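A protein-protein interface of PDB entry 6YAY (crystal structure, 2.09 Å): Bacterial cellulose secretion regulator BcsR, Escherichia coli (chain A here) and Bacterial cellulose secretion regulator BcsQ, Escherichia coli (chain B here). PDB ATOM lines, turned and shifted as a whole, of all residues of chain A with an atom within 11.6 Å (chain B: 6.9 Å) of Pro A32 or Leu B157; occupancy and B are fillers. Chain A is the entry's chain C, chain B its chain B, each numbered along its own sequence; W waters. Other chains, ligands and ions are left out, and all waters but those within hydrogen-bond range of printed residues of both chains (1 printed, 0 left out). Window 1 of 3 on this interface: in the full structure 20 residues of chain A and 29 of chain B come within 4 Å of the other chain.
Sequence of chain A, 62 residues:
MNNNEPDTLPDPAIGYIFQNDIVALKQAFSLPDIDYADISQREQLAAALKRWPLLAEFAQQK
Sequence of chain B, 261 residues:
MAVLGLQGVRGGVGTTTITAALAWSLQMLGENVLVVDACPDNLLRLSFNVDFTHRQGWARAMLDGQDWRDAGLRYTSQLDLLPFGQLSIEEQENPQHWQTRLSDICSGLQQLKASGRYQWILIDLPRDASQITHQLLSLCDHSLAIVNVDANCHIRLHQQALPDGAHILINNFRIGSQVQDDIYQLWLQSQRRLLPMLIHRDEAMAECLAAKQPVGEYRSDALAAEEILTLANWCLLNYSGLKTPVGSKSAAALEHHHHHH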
ATOM      1  N   ALA A  28     -34.312  22.138 -37.705  1.00  0.00           N
ATOM      2  CA  ALA A  28     -33.728  20.807 -37.654  1.00  0.00           C
ATOM      3  C   ALA A  28     -33.335  20.452 -36.226  1.00  0.00           C
ATOM      4  O   ALA A  28     -33.042  21.326 -35.406  1.00  0.00           O
ATOM      5  CB  ALA A  28     -32.507  20.711 -38.572  1.00  0.00           C
ATOM      6  N   PHE A  29     -33.332  19.153 -35.937  1.00  0.00           N
ATOM      7  CA  PHE A  29     -33.013  18.639 -34.612  1.00  0.00           C
ATOM      8  C   PHE A  29     -31.919  17.589 -34.732  1.00  0.00           C
ATOM      9  O   PHE A  29     -31.983  16.719 -35.606  1.00  0.00           O
ATOM     10  CB  PHE A  29     -34.254  18.045 -33.938  1.00  0.00           C
ATOM     11  CG  PHE A  29     -35.306  19.062 -33.604  1.00  0.00           C
ATOM     12  CD1 PHE A  29     -35.324  19.675 -32.362  1.00  0.00           C
ATOM     13  CD2 PHE A  29     -36.276  19.407 -34.531  1.00  0.00           C
ATOM     14  CE1 PHE A  29     -36.289  20.610 -32.048  1.00  0.00           C
ATOM     15  CE2 PHE A  29     -37.246  20.347 -34.226  1.00  0.00           C
ATOM     16  CZ  PHE A  29     -37.251  20.949 -32.981  1.00  0.00           C
ATOM     17  N   SER A  30     -30.919  17.674 -33.857  1.00  0.00           N
ATOM     18  CA  SER A  30     -29.796  16.750 -33.872  1.00  0.00           C
ATOM     19  C   SER A  30     -29.397  16.410 -32.443  1.00  0.00           C
ATOM     20  O   SER A  30     -29.690  17.150 -31.500  1.00  0.00           O
ATOM     21  CB  SER A  30     -28.590  17.330 -34.625  1.00  0.00           C
ATOM     22  OG  SER A  30     -28.906  17.576 -35.985  1.00  0.00           O
ATOM     23  N   LEU A  31     -28.725  15.272 -32.296  1.00  0.00           N
ATOM     24  CA  LEU A  31     -28.205  14.880 -30.999  1.00  0.00           C
ATOM     25  C   LEU A  31     -27.053  15.797 -30.593  1.00  0.00           C
ATOM     26  O   LEU A  31     -26.333  16.318 -31.450  1.00  0.00           O
ATOM     27  CB  LEU A  31     -27.730  13.430 -31.022  1.00  0.00           C
ATOM     28  CG  LEU A  31     -28.821  12.359 -31.052  1.00  0.00           C
ATOM     29  CD1 LEU A  31     -28.209  10.968 -31.027  1.00  0.00           C
ATOM     30  CD2 LEU A  31     -29.776  12.547 -29.887  1.00  0.00           C
ATOM     31  N   PRO A  32     -26.870  16.022 -29.291  1.00  0.00           N
ATOM     32  CA  PRO A  32     -25.769  16.880 -28.836  1.00  0.00           C
ATOM     33  C   PRO A  32     -24.417  16.362 -29.302  1.00  0.00           C
ATOM     34  O   PRO A  32     -24.167  15.155 -29.337  1.00  0.00           O
ATOM     35  CB  PRO A  32     -25.896  16.832 -27.310  1.00  0.00           C
ATOM     36  CG  PRO A  32     -27.340  16.550 -27.070  1.00  0.00           C
ATOM     37  CD  PRO A  32     -27.767  15.639 -28.187  1.00  0.00           C
ATOM     38  N   ASP A  33     -23.542  17.297 -29.665  1.00  0.00           N
ATOM     39  CA  ASP A  33     -22.209  16.962 -30.156  1.00  0.00           C
ATOM     40  C   ASP A  33     -21.356  16.457 -28.997  1.00  0.00           C
ATOM     41  O   ASP A  33     -20.960  17.235 -28.122  1.00  0.00           O
ATOM     42  CB  ASP A  33     -21.577  18.184 -30.818  1.00  0.00           C
ATOM     43  CG  ASP A  33     -20.346  17.838 -31.630  1.00  0.00           C
ATOM     44  OD1 ASP A  33     -20.007  16.638 -31.723  1.00  0.00           O
ATOM     45  OD2 ASP A  33     -19.716  18.768 -32.177  1.00  0.00           O
ATOM     46  N   ILE A  34     -21.076  15.155 -28.983  1.00  0.00           N
ATOM     47  CA  ILE A  34     -20.320  14.522 -27.908  1.00  0.00           C
ATOM     48  C   ILE A  34     -19.142  13.771 -28.515  1.00  0.00           C
ATOM     49  O   ILE A  34     -19.316  12.989 -29.457  1.00  0.00           O
ATOM     50  CB  ILE A  34     -21.199  13.569 -27.077  1.00  0.00           C
ATOM     51  CG1 ILE A  34     -22.463  14.289 -26.600  1.00  0.00           C
ATOM     52  CG2 ILE A  34     -20.420  13.025 -25.890  1.00  0.00           C
ATOM     53  CD1 ILE A  34     -23.394  13.421 -25.789  1.00  0.00           C
ATOM     54  N   ASP A  35     -17.949  14.002 -27.968  1.00  0.00           N
ATOM     55  CA  ASP A  35     -16.716  13.388 -28.453  1.00  0.00           C
ATOM     56  C   ASP A  35     -15.982  12.782 -27.267  1.00  0.00           C
ATOM     57  O   ASP A  35     -15.556  13.508 -26.363  1.00  0.00           O
ATOM     58  CB  ASP A  35     -15.836  14.420 -29.164  1.00  0.00           C
ATOM     59  CG  ASP A  35     -14.589  13.808 -29.778  1.00  0.00           C
ATOM     60  OD1 ASP A  35     -14.463  12.565 -29.783  1.00  0.00           O
ATOM     61  OD2 ASP A  35     -13.733  14.577 -30.263  1.00  0.00           O
ATOM     62  N   TYR A  36     -15.826  11.459 -27.275  1.00  0.00           N
ATOM     63  CA  TYR A  36     -15.203  10.730 -26.178  1.00  0.00           C
ATOM     64  C   TYR A  36     -13.777  10.284 -26.485  1.00  0.00           C
ATOM     65  O   TYR A  36     -13.227   9.458 -25.750  1.00  0.00           O
ATOM     66  CB  TYR A  36     -16.053   9.510 -25.806  1.00  0.00           C
ATOM     67  CG  TYR A  36     -17.302   9.819 -25.008  1.00  0.00           C
ATOM     68  CD1 TYR A  36     -17.224  10.455 -23.778  1.00  0.00           C
ATOM     69  CD2 TYR A  36     -18.556   9.452 -25.472  1.00  0.00           C
ATOM     70  CE1 TYR A  36     -18.351  10.725 -23.037  1.00  0.00           C
ATOM     71  CE2 TYR A  36     -19.695   9.722 -24.736  1.00  0.00           C
ATOM     72  CZ  TYR A  36     -19.583  10.360 -23.519  1.00  0.00           C
ATOM     73  OH  TYR A  36     -20.704  10.638 -22.773  1.00  0.00           O
ATOM     74  N   LEU A  54     -22.658   3.668 -15.557  1.00  0.00           N
ATOM     75  CA  LEU A  54     -23.457   4.419 -16.520  1.00  0.00           C
ATOM     76  C   LEU A  54     -22.583   5.317 -17.388  1.00  0.00           C
ATOM     77  O   LEU A  54     -22.776   5.393 -18.607  1.00  0.00           O
ATOM     78  CB  LEU A  54     -24.511   5.249 -15.791  1.00  0.00           C
ATOM     79  CG  LEU A  54     -25.412   6.114 -16.669  1.00  0.00           C
ATOM     80  CD1 LEU A  54     -26.318   5.247 -17.534  1.00  0.00           C
ATOM     81  CD2 LEU A  54     -26.224   7.079 -15.812  1.00  0.00           C
ATOM     82  N   LEU A  55     -21.616   6.007 -16.777  1.00  0.00           N
ATOM     83  CA  LEU A  55     -20.733   6.876 -17.549  1.00  0.00           C
ATOM     84  C   LEU A  55     -19.814   6.063 -18.450  1.00  0.00           C
ATOM     85  O   LEU A  55     -19.546   6.457 -19.592  1.00  0.00           O
ATOM     86  CB  LEU A  55     -19.916   7.765 -16.613  1.00  0.00           C
ATOM     87  CG  LEU A  55     -20.695   8.581 -15.582  1.00  0.00           C
ATOM     88  CD1 LEU A  55     -19.750   9.451 -14.770  1.00  0.00           C
ATOM     89  CD2 LEU A  55     -21.760   9.424 -16.251  1.00  0.00           C
ATOM     90  N   PHE A  58     -21.658   4.908 -21.811  1.00  0.00           N
ATOM     91  CA  PHE A  58     -21.699   5.867 -22.911  1.00  0.00           C
ATOM     92  C   PHE A  58     -20.309   6.169 -23.453  1.00  0.00           C
ATOM     93  O   PHE A  58     -20.162   6.471 -24.643  1.00  0.00           O
ATOM     94  CB  PHE A  58     -22.369   7.168 -22.462  1.00  0.00           C
ATOM     95  CG  PHE A  58     -23.833   7.031 -22.161  1.00  0.00           C
ATOM     96  CD1 PHE A  58     -24.744   6.808 -23.181  1.00  0.00           C
ATOM     97  CD2 PHE A  58     -24.303   7.144 -20.862  1.00  0.00           C
ATOM     98  CE1 PHE A  58     -26.096   6.687 -22.910  1.00  0.00           C
ATOM     99  CE2 PHE A  58     -25.656   7.024 -20.585  1.00  0.00           C
ATOM    100  CZ  PHE A  58     -26.552   6.795 -21.611  1.00  0.00           C
ATOM    101  N   ALA A  59     -19.281   6.094 -22.603  1.00  0.00           N
ATOM    102  CA  ALA A  59     -17.945   6.511 -23.015  1.00  0.00           C
ATOM    103  C   ALA A  59     -17.345   5.553 -24.037  1.00  0.00           C
ATOM    104  O   ALA A  59     -16.705   5.988 -25.001  1.00  0.00           O
ATOM    105  CB  ALA A  59     -17.038   6.629 -21.791  1.00  0.00           C
ATOM    106  N   VAL B   9     -33.614  20.636 -21.053  1.00  0.00           N
ATOM    107  CA  VAL B   9     -33.469  19.269 -21.541  1.00  0.00           C
ATOM    108  C   VAL B   9     -34.457  18.352 -20.827  1.00  0.00           C
ATOM    109  O   VAL B   9     -34.886  17.330 -21.379  1.00  0.00           O
ATOM    110  CB  VAL B   9     -32.002  18.822 -21.385  1.00  0.00           C
ATOM    111  CG1 VAL B   9     -31.873  17.308 -21.328  1.00  0.00           C
ATOM    112  CG2 VAL B   9     -31.174  19.379 -22.535  1.00  0.00           C
ATOM    113  N   ALA B 145     -30.002  25.259 -24.189  1.00  0.00           N
ATOM    114  CA  ALA B 145     -30.542  24.043 -23.600  1.00  0.00           C
ATOM    115  C   ALA B 145     -30.129  24.010 -22.133  1.00  0.00           C
ATOM    116  O   ALA B 145     -28.936  23.917 -21.821  1.00  0.00           O
ATOM    117  CB  ALA B 145     -30.042  22.808 -24.349  1.00  0.00           C
ATOM    118  N   VAL B 147     -29.736  22.481 -18.461  1.00  0.00           N
ATOM    119  CA  VAL B 147     -29.528  21.176 -17.851  1.00  0.00           C
ATOM    120  C   VAL B 147     -29.154  21.364 -16.390  1.00  0.00           C
ATOM    121  O   VAL B 147     -28.780  22.454 -15.950  1.00  0.00           O
ATOM    122  CB  VAL B 147     -28.424  20.356 -18.556  1.00  0.00           C
ATOM    123  CG1 VAL B 147     -28.761  20.123 -20.014  1.00  0.00           C
ATOM    124  CG2 VAL B 147     -27.080  21.062 -18.415  1.00  0.00           C
ATOM    125  N   ASN B 152     -29.608  11.855 -14.859  1.00  0.00           N
ATOM    126  CA  ASN B 152     -30.766  12.006 -15.735  1.00  0.00           C
ATOM    127  C   ASN B 152     -30.407  12.820 -16.975  1.00  0.00           C
ATOM    128  O   ASN B 152     -30.564  12.352 -18.109  1.00  0.00           O
ATOM    129  CB  ASN B 152     -31.916  12.654 -14.954  1.00  0.00           C
ATOM    130  CG  ASN B 152     -33.190  12.814 -15.780  1.00  0.00           C
ATOM    131  OD1 ASN B 152     -33.157  13.232 -16.937  1.00  0.00           O
ATOM    132  ND2 ASN B 152     -34.325  12.497 -15.171  1.00  0.00           N
ATOM    133  N   CYS B 153     -29.927  14.050 -16.778  1.00  0.00           N
ATOM    134  CA  CYS B 153     -29.554  14.883 -17.917  1.00  0.00           C
ATOM    135  C   CYS B 153     -28.427  14.253 -18.725  1.00  0.00           C
ATOM    136  O   CYS B 153     -28.404  14.362 -19.956  1.00  0.00           O
ATOM    137  CB  CYS B 153     -29.156  16.281 -17.443  1.00  0.00           C
ATOM    138  SG  CYS B 153     -30.544  17.319 -16.914  1.00  0.00           S
ATOM    139  N   HIS B 154     -27.485  13.586 -18.052  1.00  0.00           N
ATOM    140  CA  HIS B 154     -26.379  12.953 -18.765  1.00  0.00           C
ATOM    141  C   HIS B 154     -26.885  11.913 -19.758  1.00  0.00           C
ATOM    142  O   HIS B 154     -26.358  11.795 -20.871  1.00  0.00           O
ATOM    143  CB  HIS B 154     -25.407  12.320 -17.769  1.00  0.00           C
ATOM    144  CG  HIS B 154     -24.244  11.632 -18.416  1.00  0.00           C
ATOM    145  ND1 HIS B 154     -23.127  12.309 -18.854  1.00  0.00           N
ATOM    146  CD2 HIS B 154     -24.026  10.326 -18.702  1.00  0.00           C
ATOM    147  CE1 HIS B 154     -22.271  11.452 -19.380  1.00  0.00           C
ATOM    148  NE2 HIS B 154     -22.793  10.241 -19.301  1.00  0.00           N
ATOM    149  N   ILE B 155     -27.914  11.154 -19.377  1.00  0.00           N
ATOM    150  CA  ILE B 155     -28.488  10.180 -20.298  1.00  0.00           C
ATOM    151  C   ILE B 155     -29.210  10.882 -21.441  1.00  0.00           C
ATOM    152  O   ILE B 155     -29.068  10.502 -22.610  1.00  0.00           O
ATOM    153  CB  ILE B 155     -29.428   9.222 -19.547  1.00  0.00           C
ATOM    154  CG1 ILE B 155     -28.650   8.419 -18.504  1.00  0.00           C
ATOM    155  CG2 ILE B 155     -30.130   8.300 -20.532  1.00  0.00           C
ATOM    156  CD1 ILE B 155     -29.511   7.891 -17.369  1.00  0.00           C
ATOM    157  N   ARG B 156     -29.999  11.914 -21.124  1.00  0.00           N
ATOM    158  CA  ARG B 156     -30.808  12.575 -22.144  1.00  0.00           C
ATOM    159  C   ARG B 156     -29.949  13.180 -23.246  1.00  0.00           C
ATOM    160  O   ARG B 156     -30.360  13.192 -24.412  1.00  0.00           O
ATOM    161  CB  ARG B 156     -31.689  13.650 -21.503  1.00  0.00           C
ATOM    162  CG  ARG B 156     -32.849  13.107 -20.675  1.00  0.00           C
ATOM    163  CD  ARG B 156     -33.590  14.234 -19.973  1.00  0.00           C
ATOM    164  NE  ARG B 156     -34.767  13.766 -19.247  1.00  0.00           N
ATOM    165  CZ  ARG B 156     -35.985  13.692 -19.774  1.00  0.00           C
ATOM    166  NH1 ARG B 156     -36.184  14.047 -21.036  1.00  0.00           N
ATOM    167  NH2 ARG B 156     -37.005  13.264 -19.044  1.00  0.00           N
ATOM    168  N   LEU B 157     -28.755  13.673 -22.906  1.00  0.00           N
ATOM    169  CA  LEU B 157     -27.864  14.247 -23.908  1.00  0.00           C
ATOM    170  C   LEU B 157     -27.352  13.218 -24.909  1.00  0.00           C
ATOM    171  O   LEU B 157     -26.786  13.608 -25.936  1.00  0.00           O
ATOM    172  CB  LEU B 157     -26.680  14.933 -23.226  1.00  0.00           C
ATOM    173  CG  LEU B 157     -27.008  16.166 -22.380  1.00  0.00           C
ATOM    174  CD1 LEU B 157     -25.740  16.779 -21.791  1.00  0.00           C
ATOM    175  CD2 LEU B 157     -27.767  17.190 -23.206  1.00  0.00           C
ATOM    176  N   HIS B 158     -27.532  11.927 -24.640  1.00  0.00           N
ATOM    177  CA  HIS B 158     -27.126  10.874 -25.559  1.00  0.00           C
ATOM    178  C   HIS B 158     -28.285  10.303 -26.364  1.00  0.00           C
ATOM    179  O   HIS B 158     -28.058   9.448 -27.227  1.00  0.00           O
ATOM    180  CB  HIS B 158     -26.433   9.738 -24.796  1.00  0.00           C
ATOM    181  CG  HIS B 158     -25.118  10.127 -24.197  1.00  0.00           C
ATOM    182  ND1 HIS B 158     -25.017  10.905 -23.065  1.00  0.00           N
ATOM    183  CD2 HIS B 158     -23.849   9.843 -24.574  1.00  0.00           C
ATOM    184  CE1 HIS B 158     -23.742  11.085 -22.769  1.00  0.00           C
ATOM    185  NE2 HIS B 158     -23.011  10.449 -23.669  1.00  0.00           N
ATOM    186  N   GLN B 159     -29.518  10.745 -26.114  1.00  0.00           N
ATOM    187  CA  GLN B 159     -30.655  10.121 -26.784  1.00  0.00           C
ATOM    188  C   GLN B 159     -31.686  11.093 -27.349  1.00  0.00           C
ATOM    189  O   GLN B 159     -32.328  10.748 -28.345  1.00  0.00           O
ATOM    190  CB  GLN B 159     -31.360   9.146 -25.836  1.00  0.00           C
ATOM    191  CG  GLN B 159     -32.024   9.791 -24.638  1.00  0.00           C
ATOM    192  CD  GLN B 159     -32.763   8.778 -23.789  1.00  0.00           C
ATOM    193  OE1 GLN B 159     -32.571   7.573 -23.942  1.00  0.00           O
ATOM    194  NE2 GLN B 159     -33.619   9.262 -22.896  1.00  0.00           N
ATOM    195  N   GLN B 160     -31.880  12.277 -26.776  1.00  0.00           N
ATOM    196  CA  GLN B 160     -32.887  13.194 -27.286  1.00  0.00           C
ATOM    197  C   GLN B 160     -32.229  14.316 -28.077  1.00  0.00           C
ATOM    198  O   GLN B 160     -31.114  14.749 -27.775  1.00  0.00           O
ATOM    199  CB  GLN B 160     -33.749  13.768 -26.157  1.00  0.00           C
ATOM    200  CG  GLN B 160     -33.134  14.904 -25.374  1.00  0.00           C
ATOM    201  CD  GLN B 160     -33.993  15.319 -24.196  1.00  0.00           C
ATOM    202  OE1 GLN B 160     -34.440  14.478 -23.416  1.00  0.00           O
ATOM    203  NE2 GLN B 160     -34.228  16.618 -24.061  1.00  0.00           N
ATOM    204  N   ALA B 161     -32.929  14.768 -29.110  1.00  0.00           N
ATOM    205  CA  ALA B 161     -32.401  15.798 -29.988  1.00  0.00           C
ATOM    206  C   ALA B 161     -32.601  17.178 -29.380  1.00  0.00           C
ATOM    207  O   ALA B 161     -33.577  17.438 -28.670  1.00  0.00           O
ATOM    208  CB  ALA B 161     -33.072  15.732 -31.360  1.00  0.00           C
ATOM    209  N   LEU B 162     -31.655  18.061 -29.662  1.00  0.00           N
ATOM    210  CA  LEU B 162     -31.726  19.462 -29.296  1.00  0.00           C
ATOM    211  C   LEU B 162     -31.857  20.322 -30.547  1.00  0.00           C
ATOM    212  O   LEU B 162     -31.607  19.853 -31.663  1.00  0.00           O
ATOM    213  CB  LEU B 162     -30.477  19.878 -28.508  1.00  0.00           C
ATOM    214  CG  LEU B 162     -30.200  19.106 -27.218  1.00  0.00           C
ATOM    215  CD1 LEU B 162     -29.111  19.798 -26.413  1.00  0.00           C
ATOM    216  CD2 LEU B 162     -31.475  18.943 -26.396  1.00  0.00           C
ATOM    217  N   ILE B 168     -25.396  24.453 -24.346  1.00  0.00           N
ATOM    218  CA  ILE B 168     -25.878  23.832 -23.118  1.00  0.00           C
ATOM    219  C   ILE B 168     -25.471  24.695 -21.931  1.00  0.00           C
ATOM    220  O   ILE B 168     -24.297  25.058 -21.790  1.00  0.00           O
ATOM    221  CB  ILE B 168     -25.325  22.403 -22.979  1.00  0.00           C
ATOM    222  CG1 ILE B 168     -25.769  21.553 -24.171  1.00  0.00           C
ATOM    223  CG2 ILE B 168     -25.770  21.781 -21.670  1.00  0.00           C
ATOM    224  CD1 ILE B 168     -25.055  20.229 -24.276  1.00  0.00           C
ATOM    225  N   TRP B 187     -18.053  16.056 -18.658  1.00  0.00           N
ATOM    226  CA  TRP B 187     -18.615  16.978 -19.642  1.00  0.00           C
ATOM    227  C   TRP B 187     -17.573  17.976 -20.129  1.00  0.00           C
ATOM    228  O   TRP B 187     -17.578  18.362 -21.303  1.00  0.00           O
ATOM    229  CB  TRP B 187     -19.817  17.718 -19.054  1.00  0.00           C
ATOM    230  CG  TRP B 187     -21.048  16.878 -18.906  1.00  0.00           C
ATOM    231  CD1 TRP B 187     -21.165  15.541 -19.157  1.00  0.00           C
ATOM    232  CD2 TRP B 187     -22.341  17.321 -18.475  1.00  0.00           C
ATOM    233  NE1 TRP B 187     -22.450  15.125 -18.906  1.00  0.00           N
ATOM    234  CE2 TRP B 187     -23.192  16.198 -18.489  1.00  0.00           C
ATOM    235  CE3 TRP B 187     -22.860  18.558 -18.082  1.00  0.00           C
ATOM    236  CZ2 TRP B 187     -24.536  16.275 -18.123  1.00  0.00           C
ATOM    237  CZ3 TRP B 187     -24.194  18.632 -17.719  1.00  0.00           C
ATOM    238  CH2 TRP B 187     -25.017  17.497 -17.741  1.00  0.00           C
ATOM    239  N   GLN B 191     -18.421  17.164 -23.918  1.00  0.00           N
ATOM    240  CA  GLN B 191     -19.559  17.930 -24.423  1.00  0.00           C
ATOM    241  C   GLN B 191     -19.036  19.137 -25.193  1.00  0.00           C
ATOM    242  O   GLN B 191     -18.641  20.144 -24.602  1.00  0.00           O
ATOM    243  CB  GLN B 191     -20.471  18.351 -23.277  1.00  0.00           C
ATOM    244  CG  GLN B 191     -21.088  17.188 -22.514  1.00  0.00           C
ATOM    245  CD  GLN B 191     -22.162  16.464 -23.308  1.00  0.00           C
ATOM    246  OE1 GLN B 191     -22.713  17.002 -24.269  1.00  0.00           O
ATOM    247  NE2 GLN B 191     -22.465  15.236 -22.905  1.00  0.00           N
ATOM    248  N   ARG B 192     -19.048  19.043 -26.526  1.00  0.00           N
ATOM    249  CA  ARG B 192     -18.467  20.100 -27.349  1.00  0.00           C
ATOM    250  C   ARG B 192     -19.234  21.412 -27.233  1.00  0.00           C
ATOM    251  O   ARG B 192     -18.630  22.488 -27.321  1.00  0.00           O
ATOM    252  CB  ARG B 192     -18.410  19.665 -28.814  1.00  0.00           C
ATOM    253  CG  ARG B 192     -17.337  18.640 -29.141  1.00  0.00           C
ATOM    254  CD  ARG B 192     -16.845  18.822 -30.572  1.00  0.00           C
ATOM    255  NE  ARG B 192     -15.934  17.762 -30.994  1.00  0.00           N
ATOM    256  CZ  ARG B 192     -16.258  16.796 -31.846  1.00  0.00           C
ATOM    257  NH1 ARG B 192     -17.472  16.755 -32.378  1.00  0.00           N
ATOM    258  NH2 ARG B 192     -15.365  15.870 -32.175  1.00  0.00           N
ATOM    259  N   ARG B 193     -20.552  21.353 -27.039  1.00  0.00           N
ATOM    260  CA  ARG B 193     -21.394  22.543 -27.055  1.00  0.00           C
ATOM    261  C   ARG B 193     -21.760  23.025 -25.654  1.00  0.00           C
ATOM    262  O   ARG B 193     -22.830  23.613 -25.459  1.00  0.00           O
ATOM    263  CB  ARG B 193     -22.653  22.279 -27.881  1.00  0.00           C
ATOM    264  CG  ARG B 193     -22.361  21.646 -29.234  1.00  0.00           C
ATOM    265  CD  ARG B 193     -23.469  21.914 -30.234  1.00  0.00           C
ATOM    266  NE  ARG B 193     -23.668  23.343 -30.444  1.00  0.00           N
ATOM    267  CZ  ARG B 193     -22.910  24.095 -31.236  1.00  0.00           C
ATOM    268  NH1 ARG B 193     -21.893  23.555 -31.895  1.00  0.00           N
ATOM    269  NH2 ARG B 193     -23.168  25.389 -31.367  1.00  0.00           N
ATOM    270  N   LEU B 194     -20.886  22.802 -24.677  1.00  0.00           N
ATOM    271  CA  LEU B 194     -21.118  23.246 -23.310  1.00  0.00           C
ATOM    272  C   LEU B 194     -20.634  24.680 -23.138  1.00  0.00           C
ATOM    273  O   LEU B 194     -19.559  25.047 -23.623  1.00  0.00           O
ATOM    274  CB  LEU B 194     -20.400  22.325 -22.324  1.00  0.00           C
ATOM    275  CG  LEU B 194     -20.647  22.555 -20.833  1.00  0.00           C
ATOM    276  CD1 LEU B 194     -22.120  22.369 -20.494  1.00  0.00           C
ATOM    277  CD2 LEU B 194     -19.786  21.613 -20.013  1.00  0.00           C
HETATM  278  O   HOH W   1     -22.218  18.776 -26.195  1.00  0.00           O
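Water W1 lies within hydrogen-bond range of OE1 of Gln B191, O of Asp A33, N of Arg B193 and N of Arg B192.
Gln B159 touches Leu A31 (O to CD2, 3.5 Å). O of Gln B160 touches CD2 of Leu A31, 3.3 Å away. Pro A32 touches Gln B160 (CD to O, 3.5 Å). Gln B191 touches Asp A33. CD1 of Ile A34 touches O of Leu B157 (3.4 Å). Ile B155 touches Leu A54 (CD1 to CD2, 3.7 Å). Leu A55 touches His B154. Phe A58 touches His B154 (CD2 to NE2, 3.8 Å). CG1 of Ile B155 touches CE2 of Phe A58 (3.9 Å). His B158 touches Phe A58 (CD2 to CD1, 3.5 Å).
The side-chain hydroxyl (OH) of Tyr A36 is in hydrogen-bond range of a ring nitrogen (NE2) of His B158, at 2.5 Å. The backbone NH of Leu B162 sits at hydrogen-bond distance from the backbone carbonyl oxygen of Ser A30, at 2.8 Å. The guanidinium group (NH1) of Arg B192 lies within salt-bridge range of the side-chain carboxylate (OD1) of Asp A33. The guanidinium group of Arg B192 is in salt-bridge range of the side-chain carboxylate of Asp A35, 2.8 Å away.
The side-chain amide nitrogen (NE2) of Gln B160 sits at hydrogen-bond distance from the backbone carbonyl oxygen (O) of Val B9 (2.9 Å). The backbone carbonyl oxygen of His B154 lies within hydrogen-bond range of a ring nitrogen (ND1) of His B158 (2.7 Å). ND1 of His B154 is in hydrogen-bond range of NE1 of Trp B187, 2.9 Å away. The guanidinium group (NH1) of Arg B156 sits at hydrogen-bond distance from the side-chain amide oxygen (OE1) of Gln B160. The backbone NH (N) of Ile B168 sits at hydrogen-bond distance from the backbone carbonyl oxygen (O) of Arg B193, at 2.9 Å.
Of chain B, only Leu B157, Gln B160 and Leu B162 come within 4 Å of Pro A32. Printed residues of chain B within 4 Å of Ile A34: Leu B157 (3.4 Å), His B158 (3.7 Å) and Gln B191 (3.5 Å). Of the printed residues of chain B, Leu A54 touches Ile B155. Printed residues of chain B within 4 Å of Leu A55: His B154 (3.3 Å). Val B9 touches none of the printed residues of chain A. Printed residues of chain A within 4 Å of Ile B155: Leu A54 and Phe A58. Of chain A, only Pro A32 and Ile A34 come within 4 Å of Leu B157. Of chain A, only Ile A34 (3.7 Å), Tyr A36 (2.5 Å) and Phe A58 (3.5 Å) come within 4 Å of His B158. Of chain A, only Leu A31 (3.5 Å) comes within 4 Å of Gln B159. Gln B160 touches just these residues of chain A: Leu A31 and Pro A32. Ala B161 touches three residues of chain A. Of the printed residues of chain A, Arg B193 touches Asp A33 (3.9 Å).
Of the 20 printed residues of chain B, 11 touch a printed residue of chain A. Printed residues of chain B that touch a printed residue of chain A: His B154, Ile B155, Leu B157, His B158, Gln B159, Gln B160, Ala B161, Leu B162, Gln B191, Arg B192 and Arg B193. Hydrophobic or aromatic side chains of chain B that line the printed part of chain A: His B154, Ile B155, Leu B157, His B158, Ala B161 and Leu B162. Among the printed residues, 24 pairs touch across the chains. Among the printed residues, Asp or Glu carboxylates within 4 Å of a Lys or Arg side-chain nitrogen of the other chain: Asp A33 with Arg B192 (2.6 Å) and Asp A35 with Arg B192 (2.8 Å).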
